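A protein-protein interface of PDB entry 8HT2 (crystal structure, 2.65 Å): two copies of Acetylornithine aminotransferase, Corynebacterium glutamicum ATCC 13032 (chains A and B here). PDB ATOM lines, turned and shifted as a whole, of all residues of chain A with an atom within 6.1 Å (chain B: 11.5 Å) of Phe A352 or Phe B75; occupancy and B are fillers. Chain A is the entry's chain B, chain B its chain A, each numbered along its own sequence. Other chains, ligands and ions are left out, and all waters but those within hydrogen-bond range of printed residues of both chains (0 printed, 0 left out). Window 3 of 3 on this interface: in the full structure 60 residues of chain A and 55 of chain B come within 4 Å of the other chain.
NE of Arg B78 lies within salt-bridge range of OE1 of Glu A21, at 3.8 Å.
O of Ala B76 lies close to OE2 of Glu A21 (3.1 Å).
The backbone carbonyl oxygen (O) of Ala B76 lies within hydrogen-bond range of the backbone NH (N) of Leu A22, at 3.0 Å.
Among the printed residues, pairs that only touch across the chains: Ile A357 with Phe B75 (3.5 Å), Val A20 with Ala B76 (3.6 Å), Glu A21 with Ser B77 (3.7 Å), Phe A352 with Phe B75 (3.8 Å), Val A20 with Phe B75 (3.9 Å), Leu A22 with Leu B68 (3.9 Å), Leu A22 with Ser B77 (3.9 Å) and Leu A22 with Phe B75 (3.9 Å).
Printed residues of chain B within 4 Å of Glu A21: Ala B76, Ser B77 and Arg B78.
Of chain B, only Leu B68 (3.9 Å), Phe B75 (3.9 Å), Ala B76 (3.0 Å) and Ser B77 (3.9 Å) come within 4 Å of Leu A22.
No residue of chain B comes within 4 Å of Gly A351.
No residue of chain B comes within 4 Å of Lys A353.
No residue of chain B comes within 4 Å of Gly A355.
Ile A357 touches just one residue of chain B: Phe B75.
Of the printed residues of chain A, Leu B68 touches Leu A22 (3.9 Å).
Val B71 touches none of the printed residues of chain A.
Of chain A, only Val A20 (3.9 Å), Leu A22 (3.9 Å), Phe A352 (3.8 Å) and Ile A357 (3.5 Å) come within 4 Å of Phe B75.
Printed residues of chain A within 4 Å of Ala B76: Val A20, Glu A21 and Leu A22.
Of the printed residues of chain A, Arg B78 touches Glu A21.
Val B81 touches none of the printed residues of chain A.
The nearest residue of chain B that does not touch Phe A352 is Leu B74 (6.8 Å).
The nearest residue of chain A that does not touch Phe B75 is Leu A42 (4.1 Å).
Printed residues of chain B that touch a printed residue of chain A: Leu B68, Phe B75, Ala B76, Ser B77 and Arg B78.
Hydrophobic or aromatic side chains of chain B that line the printed part of chain A: Leu B68, Phe B75 and Ala B76.
Of the 17 printed residues of chain A, 5 touch a printed residue of chain B.
Among the printed residues, Asp or Glu carboxylates within 4 Å of a Lys or Arg side-chain nitrogen of the other chain: Glu A21 with Arg B78 (3.8 Å).
No position is printed for both chains.
Of the 11 pairs that touch across the chains among the printed residues, none has its exchanged pair printed and touching as well.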
ATOM      1  N   VAL A  20     -29.203 -11.350 -23.315  1.00  0.00           N
ATOM      2  CA  VAL A  20     -30.413 -11.823 -22.573  1.00  0.00           C
ATOM      3  C   VAL A  20     -30.848 -10.720 -21.590  1.00  0.00           C
ATOM      4  O   VAL A  20     -30.027  -9.826 -21.333  1.00  0.00           O
ATOM      5  CB  VAL A  20     -30.158 -13.177 -21.875  1.00  0.00           C
ATOM      6  CG1 VAL A  20     -29.427 -14.159 -22.787  1.00  0.00           C
ATOM      7  CG2 VAL A  20     -29.415 -13.024 -20.552  1.00  0.00           C
ATOM      8  N   GLU A  21     -32.059 -10.844 -21.026  1.00  0.00           N
ATOM      9  CA  GLU A  21     -32.938  -9.748 -20.498  1.00  0.00           C
ATOM     10  C   GLU A  21     -32.419  -9.207 -19.150  1.00  0.00           C
ATOM     11  O   GLU A  21     -31.839  -9.995 -18.384  1.00  0.00           O
ATOM     12  CB  GLU A  21     -34.379 -10.280 -20.414  1.00  0.00           C
ATOM     13  CG  GLU A  21     -35.362  -9.441 -19.600  1.00  0.00           C
ATOM     14  CD  GLU A  21     -35.815  -8.125 -20.208  1.00  0.00           C
ATOM     15  OE1 GLU A  21     -36.752  -7.506 -19.650  1.00  0.00           O
ATOM     16  OE2 GLU A  21     -35.236  -7.721 -21.233  1.00  0.00           O
ATOM     17  N   LEU A  22     -32.638  -7.906 -18.883  1.00  0.00           N
ATOM     18  CA  LEU A  22     -32.190  -7.165 -17.666  1.00  0.00           C
ATOM     19  C   LEU A  22     -33.280  -6.188 -17.222  1.00  0.00           C
ATOM     20  O   LEU A  22     -33.840  -5.532 -18.112  1.00  0.00           O
ATOM     21  CB  LEU A  22     -30.899  -6.398 -17.974  1.00  0.00           C
ATOM     22  CG  LEU A  22     -29.591  -7.121 -17.648  1.00  0.00           C
ATOM     23  CD1 LEU A  22     -28.403  -6.172 -17.739  1.00  0.00           C
ATOM     24  CD2 LEU A  22     -29.639  -7.764 -16.270  1.00  0.00           C
ATOM     25  N   TYR A  38     -25.956 -10.246 -10.468  1.00  0.00           N
ATOM     26  CA  TYR A  38     -24.611 -10.309 -11.089  1.00  0.00           C
ATOM     27  C   TYR A  38     -23.761  -9.133 -10.601  1.00  0.00           C
ATOM     28  O   TYR A  38     -24.304  -8.006 -10.483  1.00  0.00           O
ATOM     29  CB  TYR A  38     -24.718 -10.224 -12.610  1.00  0.00           C
ATOM     30  CG  TYR A  38     -25.503 -11.325 -13.273  1.00  0.00           C
ATOM     31  CD1 TYR A  38     -24.928 -12.558 -13.547  1.00  0.00           C
ATOM     32  CD2 TYR A  38     -26.815 -11.118 -13.670  1.00  0.00           C
ATOM     33  CE1 TYR A  38     -25.642 -13.563 -14.184  1.00  0.00           C
ATOM     34  CE2 TYR A  38     -27.539 -12.108 -14.312  1.00  0.00           C
ATOM     35  CZ  TYR A  38     -26.951 -13.335 -14.568  1.00  0.00           C
ATOM     36  OH  TYR A  38     -27.672 -14.305 -15.187  1.00  0.00           O
ATOM     37  N   LEU A  42     -18.744  -4.275 -16.283  1.00  0.00           N
ATOM     38  CA  LEU A  42     -18.788  -3.741 -17.663  1.00  0.00           C
ATOM     39  C   LEU A  42     -19.472  -2.374 -17.642  1.00  0.00           C
ATOM     40  O   LEU A  42     -19.067  -1.504 -18.411  1.00  0.00           O
ATOM     41  CB  LEU A  42     -19.542  -4.736 -18.546  1.00  0.00           C
ATOM     42  CG  LEU A  42     -19.694  -4.337 -20.012  1.00  0.00           C
ATOM     43  CD1 LEU A  42     -18.339  -4.228 -20.686  1.00  0.00           C
ATOM     44  CD2 LEU A  42     -20.581  -5.320 -20.755  1.00  0.00           C
ATOM     45  N   ALA A 347     -14.646 -17.417 -21.289  1.00  0.00           N
ATOM     46  CA  ALA A 347     -14.699 -16.877 -19.909  1.00  0.00           C
ATOM     47  C   ALA A 347     -15.928 -15.986 -19.731  1.00  0.00           C
ATOM     48  O   ALA A 347     -16.587 -16.100 -18.678  1.00  0.00           O
ATOM     49  CB  ALA A 347     -13.437 -16.108 -19.611  1.00  0.00           C
ATOM     50  N   VAL A 348     -16.216 -15.132 -20.718  1.00  0.00           N
ATOM     51  CA  VAL A 348     -17.446 -14.282 -20.738  1.00  0.00           C
ATOM     52  C   VAL A 348     -18.658 -15.198 -20.500  1.00  0.00           C
ATOM     53  O   VAL A 348     -19.288 -15.067 -19.432  1.00  0.00           O
ATOM     54  CB  VAL A 348     -17.581 -13.477 -22.052  1.00  0.00           C
ATOM     55  CG1 VAL A 348     -18.930 -12.775 -22.157  1.00  0.00           C
ATOM     56  CG2 VAL A 348     -16.446 -12.479 -22.235  1.00  0.00           C
ATOM     57  N   LEU A 349     -18.924 -16.118 -21.440  1.00  0.00           N
ATOM     58  CA  LEU A 349     -20.090 -17.041 -21.450  1.00  0.00           C
ATOM     59  C   LEU A 349     -20.196 -17.748 -20.098  1.00  0.00           C
ATOM     60  O   LEU A 349     -21.297 -17.759 -19.503  1.00  0.00           O
ATOM     61  CB  LEU A 349     -19.908 -18.093 -22.548  1.00  0.00           C
ATOM     62  CG  LEU A 349     -19.800 -17.600 -23.989  1.00  0.00           C
ATOM     63  CD1 LEU A 349     -19.582 -18.784 -24.926  1.00  0.00           C
ATOM     64  CD2 LEU A 349     -21.035 -16.804 -24.391  1.00  0.00           C
ATOM     65  N   ASP A 350     -19.097 -18.356 -19.651  1.00  0.00           N
ATOM     66  CA  ASP A 350     -19.066 -19.128 -18.383  1.00  0.00           C
ATOM     67  C   ASP A 350     -19.080 -18.145 -17.208  1.00  0.00           C
ATOM     68  O   ASP A 350     -19.494 -18.570 -16.111  1.00  0.00           O
ATOM     69  CB  ASP A 350     -17.903 -20.128 -18.361  1.00  0.00           C
ATOM     70  CG  ASP A 350     -18.313 -21.509 -18.852  1.00  0.00           C
ATOM     71  OD1 ASP A 350     -19.503 -21.872 -18.672  1.00  0.00           O
ATOM     72  OD2 ASP A 350     -17.448 -22.215 -19.412  1.00  0.00           O
ATOM     73  N   GLY A 351     -18.674 -16.887 -17.436  1.00  0.00           N
ATOM     74  CA  GLY A 351     -18.735 -15.787 -16.451  1.00  0.00           C
ATOM     75  C   GLY A 351     -20.126 -15.610 -15.862  1.00  0.00           C
ATOM     76  O   GLY A 351     -20.244 -15.445 -14.630  1.00  0.00           O
ATOM     77  N   PHE A 352     -21.159 -15.659 -16.700  1.00  0.00           N
ATOM     78  CA  PHE A 352     -22.570 -15.424 -16.297  1.00  0.00           C
ATOM     79  C   PHE A 352     -22.981 -16.447 -15.228  1.00  0.00           C
ATOM     80  O   PHE A 352     -23.544 -16.026 -14.201  1.00  0.00           O
ATOM     81  CB  PHE A 352     -23.496 -15.461 -17.516  1.00  0.00           C
ATOM     82  CG  PHE A 352     -23.276 -14.369 -18.537  1.00  0.00           C
ATOM     83  CD1 PHE A 352     -22.290 -14.489 -19.507  1.00  0.00           C
ATOM     84  CD2 PHE A 352     -24.072 -13.234 -18.548  1.00  0.00           C
ATOM     85  CE1 PHE A 352     -22.095 -13.493 -20.453  1.00  0.00           C
ATOM     86  CE2 PHE A 352     -23.876 -12.240 -19.496  1.00  0.00           C
ATOM     87  CZ  PHE A 352     -22.890 -12.370 -20.447  1.00  0.00           C
ATOM     88  N   LYS A 353     -22.684 -17.735 -15.446  1.00  0.00           N
ATOM     89  CA  LYS A 353     -23.090 -18.872 -14.568  1.00  0.00           C
ATOM     90  C   LYS A 353     -22.413 -18.755 -13.193  1.00  0.00           C
ATOM     91  O   LYS A 353     -22.927 -19.351 -12.228  1.00  0.00           O
ATOM     92  CB  LYS A 353     -22.728 -20.215 -15.213  1.00  0.00           C
ATOM     93  CG  LYS A 353     -23.348 -20.474 -16.583  1.00  0.00           C
ATOM     94  CD  LYS A 353     -22.558 -21.451 -17.445  1.00  0.00           C
ATOM     95  CE  LYS A 353     -23.210 -21.725 -18.786  1.00  0.00           C
ATOM     96  NZ  LYS A 353     -24.596 -22.238 -18.645  1.00  0.00           N
ATOM     97  N   HIS A 354     -21.296 -18.027 -13.104  1.00  0.00           N
ATOM     98  CA  HIS A 354     -20.552 -17.771 -11.841  1.00  0.00           C
ATOM     99  C   HIS A 354     -20.899 -16.389 -11.263  1.00  0.00           C
ATOM    100  O   HIS A 354     -20.290 -16.026 -10.253  1.00  0.00           O
ATOM    101  CB  HIS A 354     -19.046 -17.951 -12.079  1.00  0.00           C
ATOM    102  CG  HIS A 354     -18.648 -19.368 -12.349  1.00  0.00           C
ATOM    103  ND1 HIS A 354     -17.694 -20.029 -11.592  1.00  0.00           N
ATOM    104  CD2 HIS A 354     -19.074 -20.255 -13.276  1.00  0.00           C
ATOM    105  CE1 HIS A 354     -17.544 -21.254 -12.050  1.00  0.00           C
ATOM    106  NE2 HIS A 354     -18.381 -21.420 -13.082  1.00  0.00           N
ATOM    107  N   GLY A 355     -21.830 -15.644 -11.873  1.00  0.00           N
ATOM    108  CA  GLY A 355     -22.376 -14.378 -11.336  1.00  0.00           C
ATOM    109  C   GLY A 355     -21.514 -13.159 -11.655  1.00  0.00           C
ATOM    110  O   GLY A 355     -21.412 -12.252 -10.792  1.00  0.00           O
ATOM    111  N   VAL A 356     -20.906 -13.100 -12.843  1.00  0.00           N
ATOM    112  CA  VAL A 356     -20.144 -11.895 -13.285  1.00  0.00           C
ATOM    113  C   VAL A 356     -20.447 -11.609 -14.754  1.00  0.00           C
ATOM    114  O   VAL A 356     -20.544 -12.563 -15.537  1.00  0.00           O
ATOM    115  CB  VAL A 356     -18.626 -12.005 -13.040  1.00  0.00           C
ATOM    116  CG1 VAL A 356     -18.299 -11.988 -11.554  1.00  0.00           C
ATOM    117  CG2 VAL A 356     -17.994 -13.205 -13.734  1.00  0.00           C
ATOM    118  N   ILE A 357     -20.595 -10.321 -15.076  1.00  0.00           N
ATOM    119  CA  ILE A 357     -20.711  -9.782 -16.459  1.00  0.00           C
ATOM    120  C   ILE A 357     -19.338  -9.249 -16.885  1.00  0.00           C
ATOM    121  O   ILE A 357     -18.930  -8.192 -16.375  1.00  0.00           O
ATOM    122  CB  ILE A 357     -21.791  -8.691 -16.520  1.00  0.00           C
ATOM    123  CG1 ILE A 357     -23.140  -9.217 -16.028  1.00  0.00           C
ATOM    124  CG2 ILE A 357     -21.872  -8.115 -17.923  1.00  0.00           C
ATOM    125  CD1 ILE A 357     -24.096  -8.122 -15.594  1.00  0.00           C
ATOM    126  N   LEU A 358     -18.661  -9.973 -17.774  1.00  0.00           N
ATOM    127  CA  LEU A 358     -17.291  -9.669 -18.254  1.00  0.00           C
ATOM    128  C   LEU A 358     -17.348  -9.171 -19.696  1.00  0.00           C
ATOM    129  O   LEU A 358     -18.440  -9.130 -20.262  1.00  0.00           O
ATOM    130  CB  LEU A 358     -16.453 -10.943 -18.174  1.00  0.00           C
ATOM    131  CG  LEU A 358     -16.247 -11.515 -16.779  1.00  0.00           C
ATOM    132  CD1 LEU A 358     -15.649 -12.909 -16.867  1.00  0.00           C
ATOM    133  CD2 LEU A 358     -15.357 -10.601 -15.958  1.00  0.00           C
ATOM    134  N   LEU B  68     -33.218   1.000 -13.379  1.00  0.00           N
ATOM    135  CA  LEU B  68     -32.078   0.759 -14.300  1.00  0.00           C
ATOM    136  C   LEU B  68     -31.681   2.080 -14.970  1.00  0.00           C
ATOM    137  O   LEU B  68     -32.581   2.762 -15.507  1.00  0.00           O
ATOM    138  CB  LEU B  68     -32.515  -0.293 -15.328  1.00  0.00           C
ATOM    139  CG  LEU B  68     -31.487  -1.369 -15.668  1.00  0.00           C
ATOM    140  CD1 LEU B  68     -30.905  -1.986 -14.411  1.00  0.00           C
ATOM    141  CD2 LEU B  68     -32.106  -2.442 -16.551  1.00  0.00           C
ATOM    142  N   GLY B  69     -30.385   2.386 -14.979  1.00  0.00           N
ATOM    143  CA  GLY B  69     -29.908   3.600 -15.662  1.00  0.00           C
ATOM    144  C   GLY B  69     -29.649   3.332 -17.124  1.00  0.00           C
ATOM    145  O   GLY B  69     -30.525   3.618 -17.949  1.00  0.00           O
ATOM    146  N   HIS B  70     -28.452   2.856 -17.455  1.00  0.00           N
ATOM    147  CA  HIS B  70     -28.148   2.496 -18.858  1.00  0.00           C
ATOM    148  C   HIS B  70     -27.878   1.000 -18.948  1.00  0.00           C
ATOM    149  O   HIS B  70     -27.328   0.428 -18.003  1.00  0.00           O
ATOM    150  CB  HIS B  70     -26.993   3.323 -19.413  1.00  0.00           C
ATOM    151  CG  HIS B  70     -26.505   2.869 -20.748  1.00  0.00           C
ATOM    152  ND1 HIS B  70     -27.163   3.183 -21.919  1.00  0.00           N
ATOM    153  CD2 HIS B  70     -25.431   2.133 -21.103  1.00  0.00           C
ATOM    154  CE1 HIS B  70     -26.512   2.661 -22.938  1.00  0.00           C
ATOM    155  NE2 HIS B  70     -25.447   2.014 -22.462  1.00  0.00           N
ATOM    156  N   VAL B  71     -28.272   0.422 -20.071  1.00  0.00           N
ATOM    157  CA  VAL B  71     -27.908  -0.972 -20.437  1.00  0.00           C
ATOM    158  C   VAL B  71     -27.378  -0.921 -21.867  1.00  0.00           C
ATOM    159  O   VAL B  71     -28.054  -0.294 -22.718  1.00  0.00           O
ATOM    160  CB  VAL B  71     -29.111  -1.921 -20.298  1.00  0.00           C
ATOM    161  CG1 VAL B  71     -28.819  -3.286 -20.906  1.00  0.00           C
ATOM    162  CG2 VAL B  71     -29.552  -2.052 -18.849  1.00  0.00           C
ATOM    163  N   SER B  72     -26.251  -1.595 -22.088  1.00  0.00           N
ATOM    164  CA  SER B  72     -25.560  -1.741 -23.389  1.00  0.00           C
ATOM    165  C   SER B  72     -26.406  -2.538 -24.383  1.00  0.00           C
ATOM    166  O   SER B  72     -27.211  -3.367 -23.949  1.00  0.00           O
ATOM    167  CB  SER B  72     -24.233  -2.400 -23.183  1.00  0.00           C
ATOM    168  OG  SER B  72     -24.379  -3.629 -22.496  1.00  0.00           O
ATOM    169  N   ASN B  73     -26.177  -2.287 -25.674  1.00  0.00           N
ATOM    170  CA  ASN B  73     -26.813  -3.025 -26.797  1.00  0.00           C
ATOM    171  C   ASN B  73     -26.564  -4.533 -26.654  1.00  0.00           C
ATOM    172  O   ASN B  73     -27.291  -5.310 -27.288  1.00  0.00           O
ATOM    173  CB  ASN B  73     -26.288  -2.497 -28.131  1.00  0.00           C
ATOM    174  CG  ASN B  73     -26.766  -1.085 -28.395  1.00  0.00           C
ATOM    175  OD1 ASN B  73     -26.102  -0.117 -28.023  1.00  0.00           O
ATOM    176  ND2 ASN B  73     -27.941  -0.962 -28.995  1.00  0.00           N
ATOM    177  N   LEU B  74     -25.581  -4.918 -25.836  1.00  0.00           N
ATOM    178  CA  LEU B  74     -25.158  -6.322 -25.604  1.00  0.00           C
ATOM    179  C   LEU B  74     -26.225  -7.065 -24.772  1.00  0.00           C
ATOM    180  O   LEU B  74     -26.201  -8.322 -24.743  1.00  0.00           O
ATOM    181  CB  LEU B  74     -23.780  -6.304 -24.924  1.00  0.00           C
ATOM    182  CG  LEU B  74     -22.577  -6.036 -25.840  1.00  0.00           C
ATOM    183  CD1 LEU B  74     -22.621  -4.640 -26.446  1.00  0.00           C
ATOM    184  CD2 LEU B  74     -21.263  -6.245 -25.100  1.00  0.00           C
ATOM    185  N   PHE B  75     -27.143  -6.332 -24.131  1.00  0.00           N
ATOM    186  CA  PHE B  75     -28.235  -6.886 -23.283  1.00  0.00           C
ATOM    187  C   PHE B  75     -29.579  -6.293 -23.714  1.00  0.00           C
ATOM    188  O   PHE B  75     -29.595  -5.256 -24.418  1.00  0.00           O
ATOM    189  CB  PHE B  75     -27.954  -6.597 -21.808  1.00  0.00           C
ATOM    190  CG  PHE B  75     -26.629  -7.131 -21.336  1.00  0.00           C
ATOM    191  CD1 PHE B  75     -25.443  -6.540 -21.743  1.00  0.00           C
ATOM    192  CD2 PHE B  75     -26.565  -8.255 -20.525  1.00  0.00           C
ATOM    193  CE1 PHE B  75     -24.220  -7.051 -21.335  1.00  0.00           C
ATOM    194  CE2 PHE B  75     -25.342  -8.769 -20.123  1.00  0.00           C
ATOM    195  CZ  PHE B  75     -24.172  -8.161 -20.522  1.00  0.00           C
ATOM    196  N   ALA B  76     -30.675  -6.926 -23.296  1.00  0.00           N
ATOM    197  CA  ALA B  76     -32.053  -6.545 -23.678  1.00  0.00           C
ATOM    198  C   ALA B  76     -32.726  -5.849 -22.492  1.00  0.00           C
ATOM    199  O   ALA B  76     -32.462  -6.252 -21.352  1.00  0.00           O
ATOM    200  CB  ALA B  76     -32.807  -7.774 -24.137  1.00  0.00           C
ATOM    201  N   SER B  77     -33.491  -4.792 -22.759  1.00  0.00           N
ATOM    202  CA  SER B  77     -34.220  -4.045 -21.703  1.00  0.00           C
ATOM    203  C   SER B  77     -35.650  -3.818 -22.186  1.00  0.00           C
ATOM    204  O   SER B  77     -35.830  -3.586 -23.387  1.00  0.00           O
ATOM    205  CB  SER B  77     -33.537  -2.756 -21.367  1.00  0.00           C
ATOM    206  OG  SER B  77     -34.418  -1.657 -21.519  1.00  0.00           O
ATOM    207  N   ARG B  78     -36.628  -3.890 -21.286  1.00  0.00           N
ATOM    208  CA  ARG B  78     -38.054  -3.795 -21.688  1.00  0.00           C
ATOM    209  C   ARG B  78     -38.405  -2.454 -22.329  1.00  0.00           C
ATOM    210  O   ARG B  78     -38.951  -2.509 -23.428  1.00  0.00           O
ATOM    211  CB  ARG B  78     -38.976  -4.130 -20.516  1.00  0.00           C
ATOM    212  CG  ARG B  78     -40.351  -4.637 -20.923  1.00  0.00           C
ATOM    213  CD  ARG B  78     -40.924  -5.592 -19.897  1.00  0.00           C
ATOM    214  NE  ARG B  78     -40.459  -6.951 -20.129  1.00  0.00           N
ATOM    215  CZ  ARG B  78     -41.167  -7.892 -20.740  1.00  0.00           C
ATOM    216  NH1 ARG B  78     -40.658  -9.101 -20.906  1.00  0.00           N
ATOM    217  NH2 ARG B  78     -42.385  -7.625 -21.177  1.00  0.00           N
ATOM    218  N   PRO B  79     -38.157  -1.264 -21.733  1.00  0.00           N
ATOM    219  CA  PRO B  79     -38.616  -0.010 -22.324  1.00  0.00           C
ATOM    220  C   PRO B  79     -38.293   0.111 -23.813  1.00  0.00           C
ATOM    221  O   PRO B  79     -39.120   0.538 -24.540  1.00  0.00           O
ATOM    222  CB  PRO B  79     -37.872   1.046 -21.513  1.00  0.00           C
ATOM    223  CG  PRO B  79     -37.757   0.435 -20.157  1.00  0.00           C
ATOM    224  CD  PRO B  79     -37.466  -1.016 -20.459  1.00  0.00           C
ATOM    225  N   VAL B  80     -37.105  -0.314 -24.213  1.00  0.00           N
ATOM    226  CA  VAL B  80     -36.688  -0.248 -25.637  1.00  0.00           C
ATOM    227  C   VAL B  80     -37.609  -1.111 -26.510  1.00  0.00           C
ATOM    228  O   VAL B  80     -38.224  -0.540 -27.404  1.00  0.00           O
ATOM    229  CB  VAL B  80     -35.202  -0.629 -25.758  1.00  0.00           C
ATOM    230  CG1 VAL B  80     -34.621  -0.269 -27.109  1.00  0.00           C
ATOM    231  CG2 VAL B  80     -34.376  -0.015 -24.639  1.00  0.00           C
ATOM    232  N   VAL B  81     -37.692  -2.425 -26.270  1.00  0.00           N
ATOM    233  CA  VAL B  81     -38.509  -3.336 -27.143  1.00  0.00           C
ATOM    234  C   VAL B  81     -39.978  -2.888 -27.088  1.00  0.00           C
ATOM    235  O   VAL B  81     -40.646  -2.873 -28.154  1.00  0.00           O
ATOM    236  CB  VAL B  81     -38.362  -4.841 -26.829  1.00  0.00           C
ATOM    237  CG1 VAL B  81     -36.905  -5.294 -26.822  1.00  0.00           C
ATOM    238  CG2 VAL B  81     -39.043  -5.255 -25.538  1.00  0.00           C
ATOM    239  N   GLU B  82     -40.449  -2.482 -25.908  1.00  0.00           N
ATOM    240  CA  GLU B  82     -41.814  -1.923 -25.712  1.00  0.00           C
ATOM    241  C   GLU B  82     -42.045  -0.780 -26.710  1.00  0.00           C
ATOM    242  O   GLU B  82     -43.089  -0.824 -27.411  1.00  0.00           O
ATOM    243  CB  GLU B  82     -41.997  -1.431 -24.278  1.00  0.00           C
ATOM    244  CG  GLU B  82     -43.438  -1.476 -23.822  1.00  0.00           C
ATOM    245  CD  GLU B  82     -43.801  -2.698 -22.993  1.00  0.00           C
ATOM    246  OE1 GLU B  82     -44.949  -3.184 -23.132  1.00  0.00           O
ATOM    247  OE2 GLU B  82     -42.945  -3.156 -22.205  1.00  0.00           O
ATOM    248  N   PHE B 106     -32.124   2.555 -32.180  1.00  0.00           N
ATOM    249  CA  PHE B 106     -32.227   3.692 -31.228  1.00  0.00           C
ATOM    250  C   PHE B 106     -30.898   4.447 -31.142  1.00  0.00           C
ATOM    251  O   PHE B 106     -29.830   3.837 -31.206  1.00  0.00           O
ATOM    252  CB  PHE B 106     -32.746   3.193 -29.881  1.00  0.00           C
ATOM    253  CG  PHE B 106     -34.209   2.849 -29.956  1.00  0.00           C
ATOM    254  CD1 PHE B 106     -35.168   3.850 -29.899  1.00  0.00           C
ATOM    255  CD2 PHE B 106     -34.618   1.541 -30.178  1.00  0.00           C
ATOM    256  CE1 PHE B 106     -36.512   3.546 -30.025  1.00  0.00           C
ATOM    257  CE2 PHE B 106     -35.964   1.238 -30.302  1.00  0.00           C
ATOM    258  CZ  PHE B 106     -36.907   2.240 -30.224  1.00  0.00           C
ATOM    259  N   ASN B 286     -30.772   5.035 -22.995  1.00  0.00           N
ATOM    260  CA  ASN B 286     -31.864   4.424 -23.784  1.00  0.00           C
ATOM    261  C   ASN B 286     -32.999   4.030 -22.839  1.00  0.00           C
ATOM    262  O   ASN B 286     -34.081   4.545 -23.035  1.00  0.00           O
ATOM    263  CB  ASN B 286     -31.365   3.308 -24.709  1.00  0.00           C
ATOM    264  CG  ASN B 286     -30.960   3.813 -26.077  1.00  0.00           C
ATOM    265  OD1 ASN B 286     -31.781   4.347 -26.817  1.00  0.00           O
ATOM    266  ND2 ASN B 286     -29.691   3.657 -26.416  1.00  0.00           N
ATOM    267  N   PRO B 287     -32.828   3.186 -21.803  1.00  0.00           N
ATOM    268  CA  PRO B 287     -33.968   2.788 -20.987  1.00  0.00           C
ATOM    269  C   PRO B 287     -34.764   3.965 -20.413  1.00  0.00           C
ATOM    270  O   PRO B 287     -35.947   3.874 -20.398  1.00  0.00           O
ATOM    271  CB  PRO B 287     -33.356   1.905 -19.892  1.00  0.00           C
ATOM    272  CG  PRO B 287     -32.085   1.381 -20.500  1.00  0.00           C
ATOM    273  CD  PRO B 287     -31.593   2.525 -21.355  1.00  0.00           C
ATOM    274  N   CYS B 290     -36.349   5.818 -23.341  1.00  0.00           N
ATOM    275  CA  CYS B 290     -37.420   4.950 -23.879  1.00  0.00           C
ATOM    276  C   CYS B 290     -38.554   4.941 -22.855  1.00  0.00           C
ATOM    277  O   CYS B 290     -39.703   4.876 -23.266  1.00  0.00           O
ATOM    278  CB  CYS B 290     -36.879   3.567 -24.206  1.00  0.00           C
ATOM    279  SG  CYS B 290     -35.855   3.519 -25.698  1.00  0.00           S
